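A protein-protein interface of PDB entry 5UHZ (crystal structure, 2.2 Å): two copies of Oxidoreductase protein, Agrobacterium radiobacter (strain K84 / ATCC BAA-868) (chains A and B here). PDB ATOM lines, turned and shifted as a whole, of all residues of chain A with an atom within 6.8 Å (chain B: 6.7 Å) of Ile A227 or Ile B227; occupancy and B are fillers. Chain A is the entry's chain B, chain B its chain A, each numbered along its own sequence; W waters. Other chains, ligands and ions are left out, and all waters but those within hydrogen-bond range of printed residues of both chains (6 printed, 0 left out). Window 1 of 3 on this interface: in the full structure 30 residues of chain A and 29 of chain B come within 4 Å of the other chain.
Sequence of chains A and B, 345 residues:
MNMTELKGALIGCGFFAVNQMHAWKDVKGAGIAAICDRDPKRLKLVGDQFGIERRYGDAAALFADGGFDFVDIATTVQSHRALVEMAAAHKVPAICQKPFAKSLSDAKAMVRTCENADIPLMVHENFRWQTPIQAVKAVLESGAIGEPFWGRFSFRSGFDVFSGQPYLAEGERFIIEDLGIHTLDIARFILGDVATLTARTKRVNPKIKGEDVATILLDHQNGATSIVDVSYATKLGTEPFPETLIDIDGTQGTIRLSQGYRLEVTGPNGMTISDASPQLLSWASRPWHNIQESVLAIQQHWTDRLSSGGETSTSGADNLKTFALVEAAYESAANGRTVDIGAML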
ATOM      1  N   TRP A 150      -3.533 -26.257 -31.581  1.00  0.00           N
ATOM      2  CA  TRP A 150      -3.248 -26.188 -30.153  1.00  0.00           C
ATOM      3  C   TRP A 150      -4.539 -26.030 -29.356  1.00  0.00           C
ATOM      4  O   TRP A 150      -5.472 -25.385 -29.813  1.00  0.00           O
ATOM      5  CB  TRP A 150      -2.291 -25.023 -29.882  1.00  0.00           C
ATOM      6  CG  TRP A 150      -1.854 -24.839 -28.452  1.00  0.00           C
ATOM      7  CD1 TRP A 150      -0.730 -25.339 -27.867  1.00  0.00           C
ATOM      8  CD2 TRP A 150      -2.519 -24.061 -27.446  1.00  0.00           C
ATOM      9  NE1 TRP A 150      -0.661 -24.941 -26.547  1.00  0.00           N
ATOM     10  CE2 TRP A 150      -1.746 -24.151 -26.266  1.00  0.00           C
ATOM     11  CE3 TRP A 150      -3.695 -23.300 -27.428  1.00  0.00           C
ATOM     12  CZ2 TRP A 150      -2.114 -23.513 -25.080  1.00  0.00           C
ATOM     13  CZ3 TRP A 150      -4.062 -22.666 -26.246  1.00  0.00           C
ATOM     14  CH2 TRP A 150      -3.272 -22.776 -25.090  1.00  0.00           C
ATOM     15  N   GLY A 151      -4.578 -26.612 -28.160  1.00  0.00           N
ATOM     16  CA  GLY A 151      -5.725 -26.477 -27.261  1.00  0.00           C
ATOM     17  C   GLY A 151      -5.354 -26.436 -25.785  1.00  0.00           C
ATOM     18  O   GLY A 151      -4.328 -26.966 -25.380  1.00  0.00           O
ATOM     19  N   ARG A 152      -6.186 -25.776 -24.986  1.00  0.00           N
ATOM     20  CA  ARG A 152      -6.120 -25.877 -23.534  1.00  0.00           C
ATOM     21  C   ARG A 152      -7.505 -26.214 -23.014  1.00  0.00           C
ATOM     22  O   ARG A 152      -8.490 -25.572 -23.398  1.00  0.00           O
ATOM     23  CB  ARG A 152      -5.642 -24.581 -22.885  1.00  0.00           C
ATOM     24  CG  ARG A 152      -5.467 -24.710 -21.381  1.00  0.00           C
ATOM     25  CD  ARG A 152      -5.315 -23.375 -20.687  1.00  0.00           C
ATOM     26  NE  ARG A 152      -5.094 -23.554 -19.247  1.00  0.00           N
ATOM     27  CZ  ARG A 152      -5.186 -22.590 -18.328  1.00  0.00           C
ATOM     28  NH1 ARG A 152      -5.488 -21.335 -18.673  1.00  0.00           N
ATOM     29  NH2 ARG A 152      -4.975 -22.876 -17.046  1.00  0.00           N
ATOM     30  N   PHE A 153      -7.557 -27.202 -22.125  1.00  0.00           N
ATOM     31  CA  PHE A 153      -8.782 -27.644 -21.481  1.00  0.00           C
ATOM     32  C   PHE A 153      -8.534 -27.576 -19.984  1.00  0.00           C
ATOM     33  O   PHE A 153      -7.771 -28.374 -19.447  1.00  0.00           O
ATOM     34  CB  PHE A 153      -9.130 -29.069 -21.932  1.00  0.00           C
ATOM     35  CG  PHE A 153      -9.212 -29.216 -23.424  1.00  0.00           C
ATOM     36  CD1 PHE A 153      -8.084 -29.552 -24.167  1.00  0.00           C
ATOM     37  CD2 PHE A 153     -10.400 -28.973 -24.090  1.00  0.00           C
ATOM     38  CE1 PHE A 153      -8.150 -29.664 -25.546  1.00  0.00           C
ATOM     39  CE2 PHE A 153     -10.472 -29.084 -25.470  1.00  0.00           C
ATOM     40  CZ  PHE A 153      -9.345 -29.426 -26.199  1.00  0.00           C
ATOM     41  N   SER A 154      -9.169 -26.612 -19.322  1.00  0.00           N
ATOM     42  CA  SER A 154      -8.834 -26.238 -17.954  1.00  0.00           C
ATOM     43  C   SER A 154     -10.039 -26.294 -17.016  1.00  0.00           C
ATOM     44  O   SER A 154     -11.131 -25.828 -17.350  1.00  0.00           O
ATOM     45  CB  SER A 154      -8.261 -24.828 -17.950  1.00  0.00           C
ATOM     46  OG  SER A 154      -7.807 -24.469 -16.665  1.00  0.00           O
ATOM     47  N   THR A 183     -12.243 -34.060 -18.456  1.00  0.00           N
ATOM     48  CA  THR A 183     -11.411 -33.117 -19.208  1.00  0.00           C
ATOM     49  C   THR A 183     -10.659 -33.797 -20.370  1.00  0.00           C
ATOM     50  O   THR A 183     -10.526 -33.223 -21.452  1.00  0.00           O
ATOM     51  CB  THR A 183     -10.396 -32.393 -18.288  1.00  0.00           C
ATOM     52  OG1 THR A 183     -10.978 -32.161 -16.998  1.00  0.00           O
ATOM     53  CG2 THR A 183      -9.961 -31.051 -18.907  1.00  0.00           C
ATOM     54  N   ALA A 187     -11.026 -33.239 -24.337  1.00  0.00           N
ATOM     55  CA  ALA A 187      -9.849 -33.065 -25.190  1.00  0.00           C
ATOM     56  C   ALA A 187      -9.916 -33.979 -26.419  1.00  0.00           C
ATOM     57  O   ALA A 187      -9.664 -33.538 -27.544  1.00  0.00           O
ATOM     58  CB  ALA A 187      -8.572 -33.314 -24.396  1.00  0.00           C
ATOM     59  N   LEU A 191     -10.439 -32.382 -30.173  1.00  0.00           N
ATOM     60  CA  LEU A 191      -9.202 -32.456 -30.976  1.00  0.00           C
ATOM     61  C   LEU A 191      -8.817 -33.850 -31.496  1.00  0.00           C
ATOM     62  O   LEU A 191      -7.778 -34.000 -32.143  1.00  0.00           O
ATOM     63  CB  LEU A 191      -8.038 -31.854 -30.174  1.00  0.00           C
ATOM     64  CG  LEU A 191      -8.112 -30.347 -29.906  1.00  0.00           C
ATOM     65  CD1 LEU A 191      -6.891 -29.903 -29.110  1.00  0.00           C
ATOM     66  CD2 LEU A 191      -8.232 -29.541 -31.192  1.00  0.00           C
ATOM     67  N   THR A 215      -1.409 -31.776 -14.339  1.00  0.00           N
ATOM     68  CA  THR A 215      -1.115 -31.070 -15.579  1.00  0.00           C
ATOM     69  C   THR A 215      -0.684 -32.131 -16.599  1.00  0.00           C
ATOM     70  O   THR A 215       0.287 -32.859 -16.366  1.00  0.00           O
ATOM     71  CB  THR A 215       0.000 -30.031 -15.363  1.00  0.00           C
ATOM     72  OG1 THR A 215      -0.356 -29.173 -14.272  1.00  0.00           O
ATOM     73  CG2 THR A 215       0.226 -29.188 -16.605  1.00  0.00           C
ATOM     74  N   ILE A 216      -1.424 -32.226 -17.709  1.00  0.00           N
ATOM     75  CA  ILE A 216      -1.216 -33.265 -18.721  1.00  0.00           C
ATOM     76  C   ILE A 216      -0.989 -32.607 -20.083  1.00  0.00           C
ATOM     77  O   ILE A 216      -1.665 -31.632 -20.425  1.00  0.00           O
ATOM     78  CB  ILE A 216      -2.425 -34.224 -18.802  1.00  0.00           C
ATOM     79  CG1 ILE A 216      -2.788 -34.765 -17.412  1.00  0.00           C
ATOM     80  CG2 ILE A 216      -2.139 -35.368 -19.771  1.00  0.00           C
ATOM     81  CD1 ILE A 216      -4.113 -35.488 -17.347  1.00  0.00           C
ATOM     82  N   LEU A 217      -0.042 -33.149 -20.850  1.00  0.00           N
ATOM     83  CA  LEU A 217       0.311 -32.639 -22.181  1.00  0.00           C
ATOM     84  C   LEU A 217       0.045 -33.735 -23.217  1.00  0.00           C
ATOM     85  O   LEU A 217       0.670 -34.797 -23.177  1.00  0.00           O
ATOM     86  CB  LEU A 217       1.777 -32.223 -22.189  1.00  0.00           C
ATOM     87  CG  LEU A 217       2.421 -31.759 -23.496  1.00  0.00           C
ATOM     88  CD1 LEU A 217       1.884 -30.403 -23.915  1.00  0.00           C
ATOM     89  CD2 LEU A 217       3.936 -31.708 -23.327  1.00  0.00           C
ATOM     90  N   LEU A 218      -0.887 -33.468 -24.132  1.00  0.00           N
ATOM     91  CA  LEU A 218      -1.368 -34.454 -25.098  1.00  0.00           C
ATOM     92  C   LEU A 218      -0.843 -34.170 -26.512  1.00  0.00           C
ATOM     93  O   LEU A 218      -0.880 -33.026 -26.980  1.00  0.00           O
ATOM     94  CB  LEU A 218      -2.902 -34.454 -25.121  1.00  0.00           C
ATOM     95  CG  LEU A 218      -3.639 -34.608 -23.792  1.00  0.00           C
ATOM     96  CD1 LEU A 218      -5.142 -34.513 -23.991  1.00  0.00           C
ATOM     97  CD2 LEU A 218      -3.301 -35.940 -23.146  1.00  0.00           C
ATOM     98  N   HIS A 220      -1.934 -35.071 -30.070  1.00  0.00           N
ATOM     99  CA  HIS A 220      -3.073 -35.627 -30.796  1.00  0.00           C
ATOM    100  C   HIS A 220      -2.623 -36.219 -32.130  1.00  0.00           C
ATOM    101  O   HIS A 220      -1.656 -35.745 -32.734  1.00  0.00           O
ATOM    102  CB  HIS A 220      -4.160 -34.564 -30.983  1.00  0.00           C
ATOM    103  CG  HIS A 220      -4.816 -34.155 -29.701  1.00  0.00           C
ATOM    104  ND1 HIS A 220      -5.967 -34.753 -29.235  1.00  0.00           N
ATOM    105  CD2 HIS A 220      -4.467 -33.234 -28.773  1.00  0.00           C
ATOM    106  CE1 HIS A 220      -6.307 -34.206 -28.080  1.00  0.00           C
ATOM    107  NE2 HIS A 220      -5.413 -33.281 -27.777  1.00  0.00           N
ATOM    108  N   THR A 225      -1.355 -30.162 -30.440  1.00  0.00           N
ATOM    109  CA  THR A 225      -0.877 -30.327 -29.075  1.00  0.00           C
ATOM    110  C   THR A 225      -1.911 -29.702 -28.140  1.00  0.00           C
ATOM    111  O   THR A 225      -2.481 -28.670 -28.465  1.00  0.00           O
ATOM    112  CB  THR A 225       0.466 -29.605 -28.868  1.00  0.00           C
ATOM    113  OG1 THR A 225       1.375 -29.944 -29.924  1.00  0.00           O
ATOM    114  CG2 THR A 225       1.071 -29.974 -27.529  1.00  0.00           C
ATOM    115  N   SER A 226      -2.163 -30.304 -26.987  1.00  0.00           N
ATOM    116  CA  SER A 226      -3.044 -29.671 -26.011  1.00  0.00           C
ATOM    117  C   SER A 226      -2.566 -29.811 -24.572  1.00  0.00           C
ATOM    118  O   SER A 226      -1.701 -30.636 -24.251  1.00  0.00           O
ATOM    119  CB  SER A 226      -4.474 -30.186 -26.144  1.00  0.00           C
ATOM    120  OG  SER A 226      -4.657 -31.397 -25.444  1.00  0.00           O
ATOM    121  N   ILE A 227      -3.140 -28.965 -23.721  1.00  0.00           N
ATOM    122  CA  ILE A 227      -2.896 -28.981 -22.295  1.00  0.00           C
ATOM    123  C   ILE A 227      -4.225 -29.291 -21.622  1.00  0.00           C
ATOM    124  O   ILE A 227      -5.241 -28.647 -21.905  1.00  0.00           O
ATOM    125  CB  ILE A 227      -2.355 -27.626 -21.818  1.00  0.00           C
ATOM    126  CG1 ILE A 227      -0.971 -27.368 -22.425  1.00  0.00           C
ATOM    127  CG2 ILE A 227      -2.269 -27.565 -20.296  1.00  0.00           C
ATOM    128  CD1 ILE A 227      -0.700 -25.904 -22.686  1.00  0.00           C
ATOM    129  N   VAL A 228      -4.214 -30.302 -20.763  1.00  0.00           N
ATOM    130  CA  VAL A 228      -5.330 -30.604 -19.885  1.00  0.00           C
ATOM    131  C   VAL A 228      -4.805 -30.349 -18.489  1.00  0.00           C
ATOM    132  O   VAL A 228      -3.998 -31.131 -17.987  1.00  0.00           O
ATOM    133  CB  VAL A 228      -5.794 -32.064 -20.034  1.00  0.00           C
ATOM    134  CG1 VAL A 228      -6.758 -32.464 -18.917  1.00  0.00           C
ATOM    135  CG2 VAL A 228      -6.413 -32.264 -21.406  1.00  0.00           C
ATOM    136  N   ASP A 229      -5.228 -29.240 -17.887  1.00  0.00           N
ATOM    137  CA  ASP A 229      -4.827 -28.891 -16.523  1.00  0.00           C
ATOM    138  C   ASP A 229      -6.055 -28.870 -15.621  1.00  0.00           C
ATOM    139  O   ASP A 229      -7.053 -28.222 -15.932  1.00  0.00           O
ATOM    140  CB  ASP A 229      -4.064 -27.563 -16.483  1.00  0.00           C
ATOM    141  CG  ASP A 229      -4.874 -26.393 -16.993  1.00  0.00           C
ATOM    142  OD1 ASP A 229      -4.990 -26.241 -18.225  1.00  0.00           O
ATOM    143  OD2 ASP A 229      -5.380 -25.610 -16.163  1.00  0.00           O
ATOM    144  N   TRP B 150       1.835 -24.365  -8.919  1.00  0.00           N
ATOM    145  CA  TRP B 150       1.501 -24.468 -10.337  1.00  0.00           C
ATOM    146  C   TRP B 150       1.594 -23.096 -10.984  1.00  0.00           C
ATOM    147  O   TRP B 150       1.255 -22.092 -10.360  1.00  0.00           O
ATOM    148  CB  TRP B 150       0.094 -25.060 -10.524  1.00  0.00           C
ATOM    149  CG  TRP B 150      -0.291 -25.273 -11.962  1.00  0.00           C
ATOM    150  CD1 TRP B 150      -0.041 -26.376 -12.720  1.00  0.00           C
ATOM    151  CD2 TRP B 150      -0.979 -24.348 -12.813  1.00  0.00           C
ATOM    152  NE1 TRP B 150      -0.533 -26.200 -13.991  1.00  0.00           N
ATOM    153  CE2 TRP B 150      -1.119 -24.965 -14.074  1.00  0.00           C
ATOM    154  CE3 TRP B 150      -1.505 -23.061 -12.626  1.00  0.00           C
ATOM    155  CZ2 TRP B 150      -1.757 -24.340 -15.149  1.00  0.00           C
ATOM    156  CZ3 TRP B 150      -2.145 -22.437 -13.699  1.00  0.00           C
ATOM    157  CH2 TRP B 150      -2.264 -23.079 -14.942  1.00  0.00           C
ATOM    158  N   GLY B 151       2.040 -23.064 -12.238  1.00  0.00           N
ATOM    159  CA  GLY B 151       2.138 -21.821 -12.992  1.00  0.00           C
ATOM    160  C   GLY B 151       1.857 -21.988 -14.475  1.00  0.00           C
ATOM    161  O   GLY B 151       1.998 -23.081 -15.020  1.00  0.00           O
ATOM    162  N   ARG B 152       1.437 -20.897 -15.117  1.00  0.00           N
ATOM    163  CA  ARG B 152       1.364 -20.827 -16.574  1.00  0.00           C
ATOM    164  C   ARG B 152       1.947 -19.505 -17.032  1.00  0.00           C
ATOM    165  O   ARG B 152       1.606 -18.458 -16.488  1.00  0.00           O
ATOM    166  CB  ARG B 152      -0.072 -20.926 -17.081  1.00  0.00           C
ATOM    167  CG  ARG B 152      -0.163 -20.982 -18.604  1.00  0.00           C
ATOM    168  CD  ARG B 152      -1.546 -20.659 -19.136  1.00  0.00           C
ATOM    169  NE  ARG B 152      -1.555 -20.755 -20.596  1.00  0.00           N
ATOM    170  CZ  ARG B 152      -2.568 -20.393 -21.383  1.00  0.00           C
ATOM    171  NH1 ARG B 152      -3.693 -19.918 -20.868  1.00  0.00           N
ATOM    172  NH2 ARG B 152      -2.455 -20.522 -22.697  1.00  0.00           N
ATOM    173  N   PHE B 153       2.794 -19.571 -18.054  1.00  0.00           N
ATOM    174  CA  PHE B 153       3.451 -18.410 -18.601  1.00  0.00           C
ATOM    175  C   PHE B 153       3.204 -18.459 -20.091  1.00  0.00           C
ATOM    176  O   PHE B 153       3.713 -19.353 -20.762  1.00  0.00           O
ATOM    177  CB  PHE B 153       4.955 -18.463 -18.308  1.00  0.00           C
ATOM    178  CG  PHE B 153       5.284 -18.561 -16.848  1.00  0.00           C
ATOM    179  CD1 PHE B 153       5.304 -19.798 -16.202  1.00  0.00           C
ATOM    180  CD2 PHE B 153       5.580 -17.423 -16.115  1.00  0.00           C
ATOM    181  CE1 PHE B 153       5.604 -19.889 -14.849  1.00  0.00           C
ATOM    182  CE2 PHE B 153       5.886 -17.506 -14.762  1.00  0.00           C
ATOM    183  CZ  PHE B 153       5.892 -18.740 -14.128  1.00  0.00           C
ATOM    184  N   SER B 154       2.430 -17.497 -20.598  1.00  0.00           N
ATOM    185  CA  SER B 154       1.869 -17.556 -21.943  1.00  0.00           C
ATOM    186  C   SER B 154       2.148 -16.292 -22.767  1.00  0.00           C
ATOM    187  O   SER B 154       1.964 -15.177 -22.292  1.00  0.00           O
ATOM    188  CB  SER B 154       0.359 -17.768 -21.850  1.00  0.00           C
ATOM    189  OG  SER B 154      -0.162 -18.239 -23.080  1.00  0.00           O
ATOM    190  N   ARG B 156       0.982 -15.730 -26.535  1.00  0.00           N
ATOM    191  CA  ARG B 156       0.306 -16.185 -27.759  1.00  0.00           C
ATOM    192  C   ARG B 156      -0.134 -14.953 -28.542  1.00  0.00           C
ATOM    193  O   ARG B 156      -0.928 -14.140 -28.032  1.00  0.00           O
ATOM    194  CB  ARG B 156      -0.909 -17.059 -27.437  1.00  0.00           C
ATOM    195  CG  ARG B 156      -0.663 -18.161 -26.417  1.00  0.00           C
ATOM    196  CD  ARG B 156      -1.781 -19.205 -26.428  1.00  0.00           C
ATOM    197  NE  ARG B 156      -1.713 -20.074 -27.608  1.00  0.00           N
ATOM    198  CZ  ARG B 156      -0.822 -21.052 -27.796  1.00  0.00           C
ATOM    199  NH1 ARG B 156       0.119 -21.326 -26.885  1.00  0.00           N
ATOM    200  NH2 ARG B 156      -0.863 -21.763 -28.918  1.00  0.00           N
ATOM    201  N   THR B 183      10.265 -16.248 -21.993  1.00  0.00           N
ATOM    202  CA  THR B 183       9.187 -16.844 -21.208  1.00  0.00           C
ATOM    203  C   THR B 183       9.726 -17.888 -20.231  1.00  0.00           C
ATOM    204  O   THR B 183       9.255 -18.003 -19.099  1.00  0.00           O
ATOM    205  CB  THR B 183       8.122 -17.488 -22.125  1.00  0.00           C
ATOM    206  OG1 THR B 183       7.939 -16.678 -23.287  1.00  0.00           O
ATOM    207  CG2 THR B 183       6.785 -17.629 -21.396  1.00  0.00           C
ATOM    208  N   ALA B 187       9.792 -17.935 -16.161  1.00  0.00           N
ATOM    209  CA  ALA B 187       9.397 -19.106 -15.371  1.00  0.00           C
ATOM    210  C   ALA B 187      10.413 -19.422 -14.283  1.00  0.00           C
ATOM    211  O   ALA B 187      10.029 -19.711 -13.150  1.00  0.00           O
ATOM    212  CB  ALA B 187       9.178 -20.314 -16.269  1.00  0.00           C
ATOM    213  N   THR B 215       4.996 -25.697 -26.835  1.00  0.00           N
ATOM    214  CA  THR B 215       4.362 -25.933 -25.548  1.00  0.00           C
ATOM    215  C   THR B 215       5.357 -26.736 -24.700  1.00  0.00           C
ATOM    216  O   THR B 215       5.787 -27.813 -25.090  1.00  0.00           O
ATOM    217  CB  THR B 215       3.027 -26.683 -25.713  1.00  0.00           C
ATOM    218  OG1 THR B 215       2.184 -25.968 -26.631  1.00  0.00           O
ATOM    219  CG2 THR B 215       2.310 -26.828 -24.376  1.00  0.00           C
ATOM    220  N   ILE B 216       5.731 -26.175 -23.556  1.00  0.00           N
ATOM    221  CA  ILE B 216       6.782 -26.714 -22.700  1.00  0.00           C
ATOM    222  C   ILE B 216       6.188 -26.921 -21.304  1.00  0.00           C
ATOM    223  O   ILE B 216       5.452 -26.067 -20.814  1.00  0.00           O
ATOM    224  CB  ILE B 216       8.000 -25.766 -22.650  1.00  0.00           C
ATOM    225  CG1 ILE B 216       8.469 -25.417 -24.068  1.00  0.00           C
ATOM    226  CG2 ILE B 216       9.149 -26.410 -21.888  1.00  0.00           C
ATOM    227  CD1 ILE B 216       9.492 -24.309 -24.138  1.00  0.00           C
ATOM    228  N   LEU B 217       6.490 -28.069 -20.701  1.00  0.00           N
ATOM    229  CA  LEU B 217       6.024 -28.439 -19.367  1.00  0.00           C
ATOM    230  C   LEU B 217       7.254 -28.555 -18.464  1.00  0.00           C
ATOM    231  O   LEU B 217       8.138 -29.376 -18.732  1.00  0.00           O
ATOM    232  CB  LEU B 217       5.291 -29.774 -19.452  1.00  0.00           C
ATOM    233  CG  LEU B 217       4.844 -30.490 -18.173  1.00  0.00           C
ATOM    234  CD1 LEU B 217       3.761 -29.695 -17.467  1.00  0.00           C
ATOM    235  CD2 LEU B 217       4.344 -31.891 -18.497  1.00  0.00           C
ATOM    236  N   LEU B 218       7.314 -27.732 -17.414  1.00  0.00           N
ATOM    237  CA  LEU B 218       8.486 -27.633 -16.537  1.00  0.00           C
ATOM    238  C   LEU B 218       8.216 -28.251 -15.168  1.00  0.00           C
ATOM    239  O   LEU B 218       7.160 -28.022 -14.583  1.00  0.00           O
ATOM    240  CB  LEU B 218       8.884 -26.165 -16.346  1.00  0.00           C
ATOM    241  CG  LEU B 218       9.129 -25.325 -17.604  1.00  0.00           C
ATOM    242  CD1 LEU B 218       9.448 -23.881 -17.246  1.00  0.00           C
ATOM    243  CD2 LEU B 218      10.257 -25.917 -18.430  1.00  0.00           C
ATOM    244  N   HIS B 220       9.821 -27.863 -11.635  1.00  0.00           N
ATOM    245  CA  HIS B 220      10.748 -27.015 -10.892  1.00  0.00           C
ATOM    246  C   HIS B 220      11.330 -27.761  -9.691  1.00  0.00           C
ATOM    247  O   HIS B 220      10.707 -28.688  -9.159  1.00  0.00           O
ATOM    248  CB  HIS B 220      10.053 -25.729 -10.454  1.00  0.00           C
ATOM    249  CG  HIS B 220       9.639 -24.856 -11.596  1.00  0.00           C
ATOM    250  ND1 HIS B 220      10.425 -23.830 -12.070  1.00  0.00           N
ATOM    251  CD2 HIS B 220       8.526 -24.868 -12.372  1.00  0.00           C
ATOM    252  CE1 HIS B 220       9.810 -23.238 -13.080  1.00  0.00           C
ATOM    253  NE2 HIS B 220       8.656 -23.849 -13.285  1.00  0.00           N
ATOM    254  N   THR B 225       4.963 -27.299 -10.759  1.00  0.00           N
ATOM    255  CA  THR B 225       4.832 -27.631 -12.167  1.00  0.00           C
ATOM    256  C   THR B 225       4.437 -26.357 -12.902  1.00  0.00           C
ATOM    257  O   THR B 225       3.679 -25.551 -12.365  1.00  0.00           O
ATOM    258  CB  THR B 225       3.726 -28.679 -12.388  1.00  0.00           C
ATOM    259  OG1 THR B 225       3.921 -29.784 -11.504  1.00  0.00           O
ATOM    260  CG2 THR B 225       3.730 -29.184 -13.818  1.00  0.00           C
ATOM    261  N   SER B 226       4.932 -26.167 -14.122  1.00  0.00           N
ATOM    262  CA  SER B 226       4.512 -25.014 -14.911  1.00  0.00           C
ATOM    263  C   SER B 226       4.460 -25.271 -16.425  1.00  0.00           C
ATOM    264  O   SER B 226       5.225 -26.067 -16.968  1.00  0.00           O
ATOM    265  CB  SER B 226       5.363 -23.783 -14.571  1.00  0.00           C
ATOM    266  OG  SER B 226       6.496 -23.689 -15.399  1.00  0.00           O
ATOM    267  N   ILE B 227       3.513 -24.599 -17.074  1.00  0.00           N
ATOM    268  CA  ILE B 227       3.365 -24.599 -18.520  1.00  0.00           C
ATOM    269  C   ILE B 227       3.994 -23.324 -19.055  1.00  0.00           C
ATOM    270  O   ILE B 227       3.682 -22.246 -18.569  1.00  0.00           O
ATOM    271  CB  ILE B 227       1.873 -24.578 -18.924  1.00  0.00           C
ATOM    272  CG1 ILE B 227       1.155 -25.844 -18.441  1.00  0.00           C
ATOM    273  CG2 ILE B 227       1.707 -24.402 -20.433  1.00  0.00           C
ATOM    274  CD1 ILE B 227       1.656 -27.124 -19.075  1.00  0.00           C
ATOM    275  N   VAL B 228       4.862 -23.445 -20.051  1.00  0.00           N
ATOM    276  CA  VAL B 228       5.304 -22.300 -20.851  1.00  0.00           C
ATOM    277  C   VAL B 228       4.799 -22.560 -22.262  1.00  0.00           C
ATOM    278  O   VAL B 228       5.262 -23.491 -22.916  1.00  0.00           O
ATOM    279  CB  VAL B 228       6.836 -22.130 -20.816  1.00  0.00           C
ATOM    280  CG1 VAL B 228       7.340 -21.209 -21.924  1.00  0.00           C
ATOM    281  CG2 VAL B 228       7.255 -21.594 -19.458  1.00  0.00           C
ATOM    282  N   ASP B 229       3.832 -21.765 -22.712  1.00  0.00           N
ATOM    283  CA  ASP B 229       3.261 -21.940 -24.036  1.00  0.00           C
ATOM    284  C   ASP B 229       3.425 -20.654 -24.829  1.00  0.00           C
ATOM    285  O   ASP B 229       3.038 -19.584 -24.370  1.00  0.00           O
ATOM    286  CB  ASP B 229       1.798 -22.396 -23.973  1.00  0.00           C
ATOM    287  CG  ASP B 229       0.878 -21.382 -23.329  1.00  0.00           C
ATOM    288  OD1 ASP B 229       0.796 -21.342 -22.088  1.00  0.00           O
ATOM    289  OD2 ASP B 229       0.208 -20.639 -24.076  1.00  0.00           O
HETATM  290  O   HOH W   1       2.871 -27.309 -29.623  1.00  0.00           O
HETATM  291  O   HOH W   2      -4.505 -18.595 -18.556  1.00  0.00           O
HETATM  292  O   HOH W   3       0.793 -30.258 -12.038  1.00  0.00           O
HETATM  293  O   HOH W   4       1.998 -23.390 -27.643  1.00  0.00           O
HETATM  294  O   HOH W   5      -2.878 -28.470 -13.084  1.00  0.00           O
HETATM  295  O   HOH W   6      -6.997 -19.989 -20.531  1.00  0.00           O
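Trp A150 touches Thr B215, and with the chains exchanged Thr A215 touches Trp B150. Trp A150 touches Asp B229, and with the chains exchanged Asp A229 touches Trp B150. Arg A152 touches its own counterpart, Arg B152. Thr A215 touches Ile B227, and with the chains exchanged Ile A227 touches Thr B215.
Water W3 lies within hydrogen-bond range of OG1 of Thr A215 and OG1 of Thr B225. Water W6 lies within hydrogen-bond range of the guanidinium group (NH1) of Arg A152 (2.7 Å) and the guanidinium group (NH1) of Arg B152 (3.3 Å). Water W4 lies within hydrogen-bond range of OG1 of Thr B215 (2.8 Å), NH1 of Arg B156 (2.9 Å) and NE1 of Trp A150 (3.3 Å). Water W2 bridges NH1 of Arg B152 (2.8 Å) and NH1 of Arg A152 (2.9 Å). Water W5 bridges OG1 of Thr A215 and NE1 of Trp B150. Water W1 bridges OG1 of Thr A225 (3.0 Å) and OG1 of Thr B215 (3.3 Å).
Of the 18 printed residues of chain A, 6 touch a printed residue of chain B. Printed residues of chain A that touch a printed residue of chain B: Trp A150, Arg A152, Thr A215, Leu A217, Ile A227 and Asp A229. Of the 18 printed residues of chain B, 7 touch a printed residue of chain A. Among the printed residues, no Asp or Glu carboxylate lies within 4 Å of a Lys or Arg side-chain nitrogen of the other chain.
Arg B152 touches Trp A150 (NH2 to CH2, 3.4 Å). Trp A150 touches Arg B156 (CD2 to NH2, 3.2 Å). OD2 of Asp B229 touches CZ2 of Trp A150, 3.8 Å away. Arg A152 touches Trp B150. Thr A215 touches Leu B217 (CG2 to CD1, 3.7 Å). CD1 of Ile B227 touches CG2 of Thr A215 (3.5 Å). Leu A217 touches Thr B215. CD1 of Ile A227 touches CG2 of Thr B215 (3.6 Å). CG2 of Ile B227 touches CD1 of Ile A227, at 3.6 Å. OD2 of Asp A229 touches CZ2 of Trp B150, 3.97 Å away.
NH1 of Arg A152 sits close to NH1 of Arg B152 (3.2 Å). The indole nitrogen (NE1) of Trp B150 lies within hydrogen-bond range of the side-chain hydroxyl (OG1) of Thr A215 (3.0 Å). OG1 of Thr B215 sits at hydrogen-bond distance from NE1 of Trp A150 (3.0 Å).
Of the printed residues of chain B, Arg A152 touches Trp B150 and Arg B152. Of the printed residues of chain B, Leu A217 touches Thr B215. Ile A227 touches just these residues of chain B: Thr B215 and Ile B227. Printed residues of chain A within 4 Å of Arg B152: Trp A150 and Arg A152. Of the printed residues of chain A, Thr B215 touches Trp A150 (3.0 Å), Leu A217 (3.6 Å) and Ile A227 (3.6 Å). Ser B226 touches none of the printed residues of chain A. Ile B227 touches just these residues of chain A: Thr A215 and Ile A227. Printed residues of chain A within 4 Å of Asp B229: Trp A150. The nearest residue of chain B that does not touch Ile A227 is Asp B229 (4.5 Å). The nearest residue of chain A that does not touch Ile B227 is Ile A216 (5.8 Å).
NE of Arg A152 is in salt-bridge range of OD1 of Asp A229 (2.9 Å). The side-chain hydroxyl of Ser B154 lies within hydrogen-bond range of the side-chain carboxylate of Asp B229 (2.6 Å). The backbone carbonyl oxygen of Phe B153 lies within hydrogen-bond range of the backbone NH of Asp B229 (3.1 Å). The side-chain carboxylate of Asp A229 lies within hydrogen-bond range of the side-chain hydroxyl of Ser A154 (2.7 Å). The backbone carbonyl oxygen (O) of Gly A151 is in hydrogen-bond range of the backbone NH (N) of Ile A227, at 2.9 Å. The guanidinium group of Arg B152 is in hydrogen-bond range of the side-chain hydroxyl of Ser B154 (3.3 Å).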
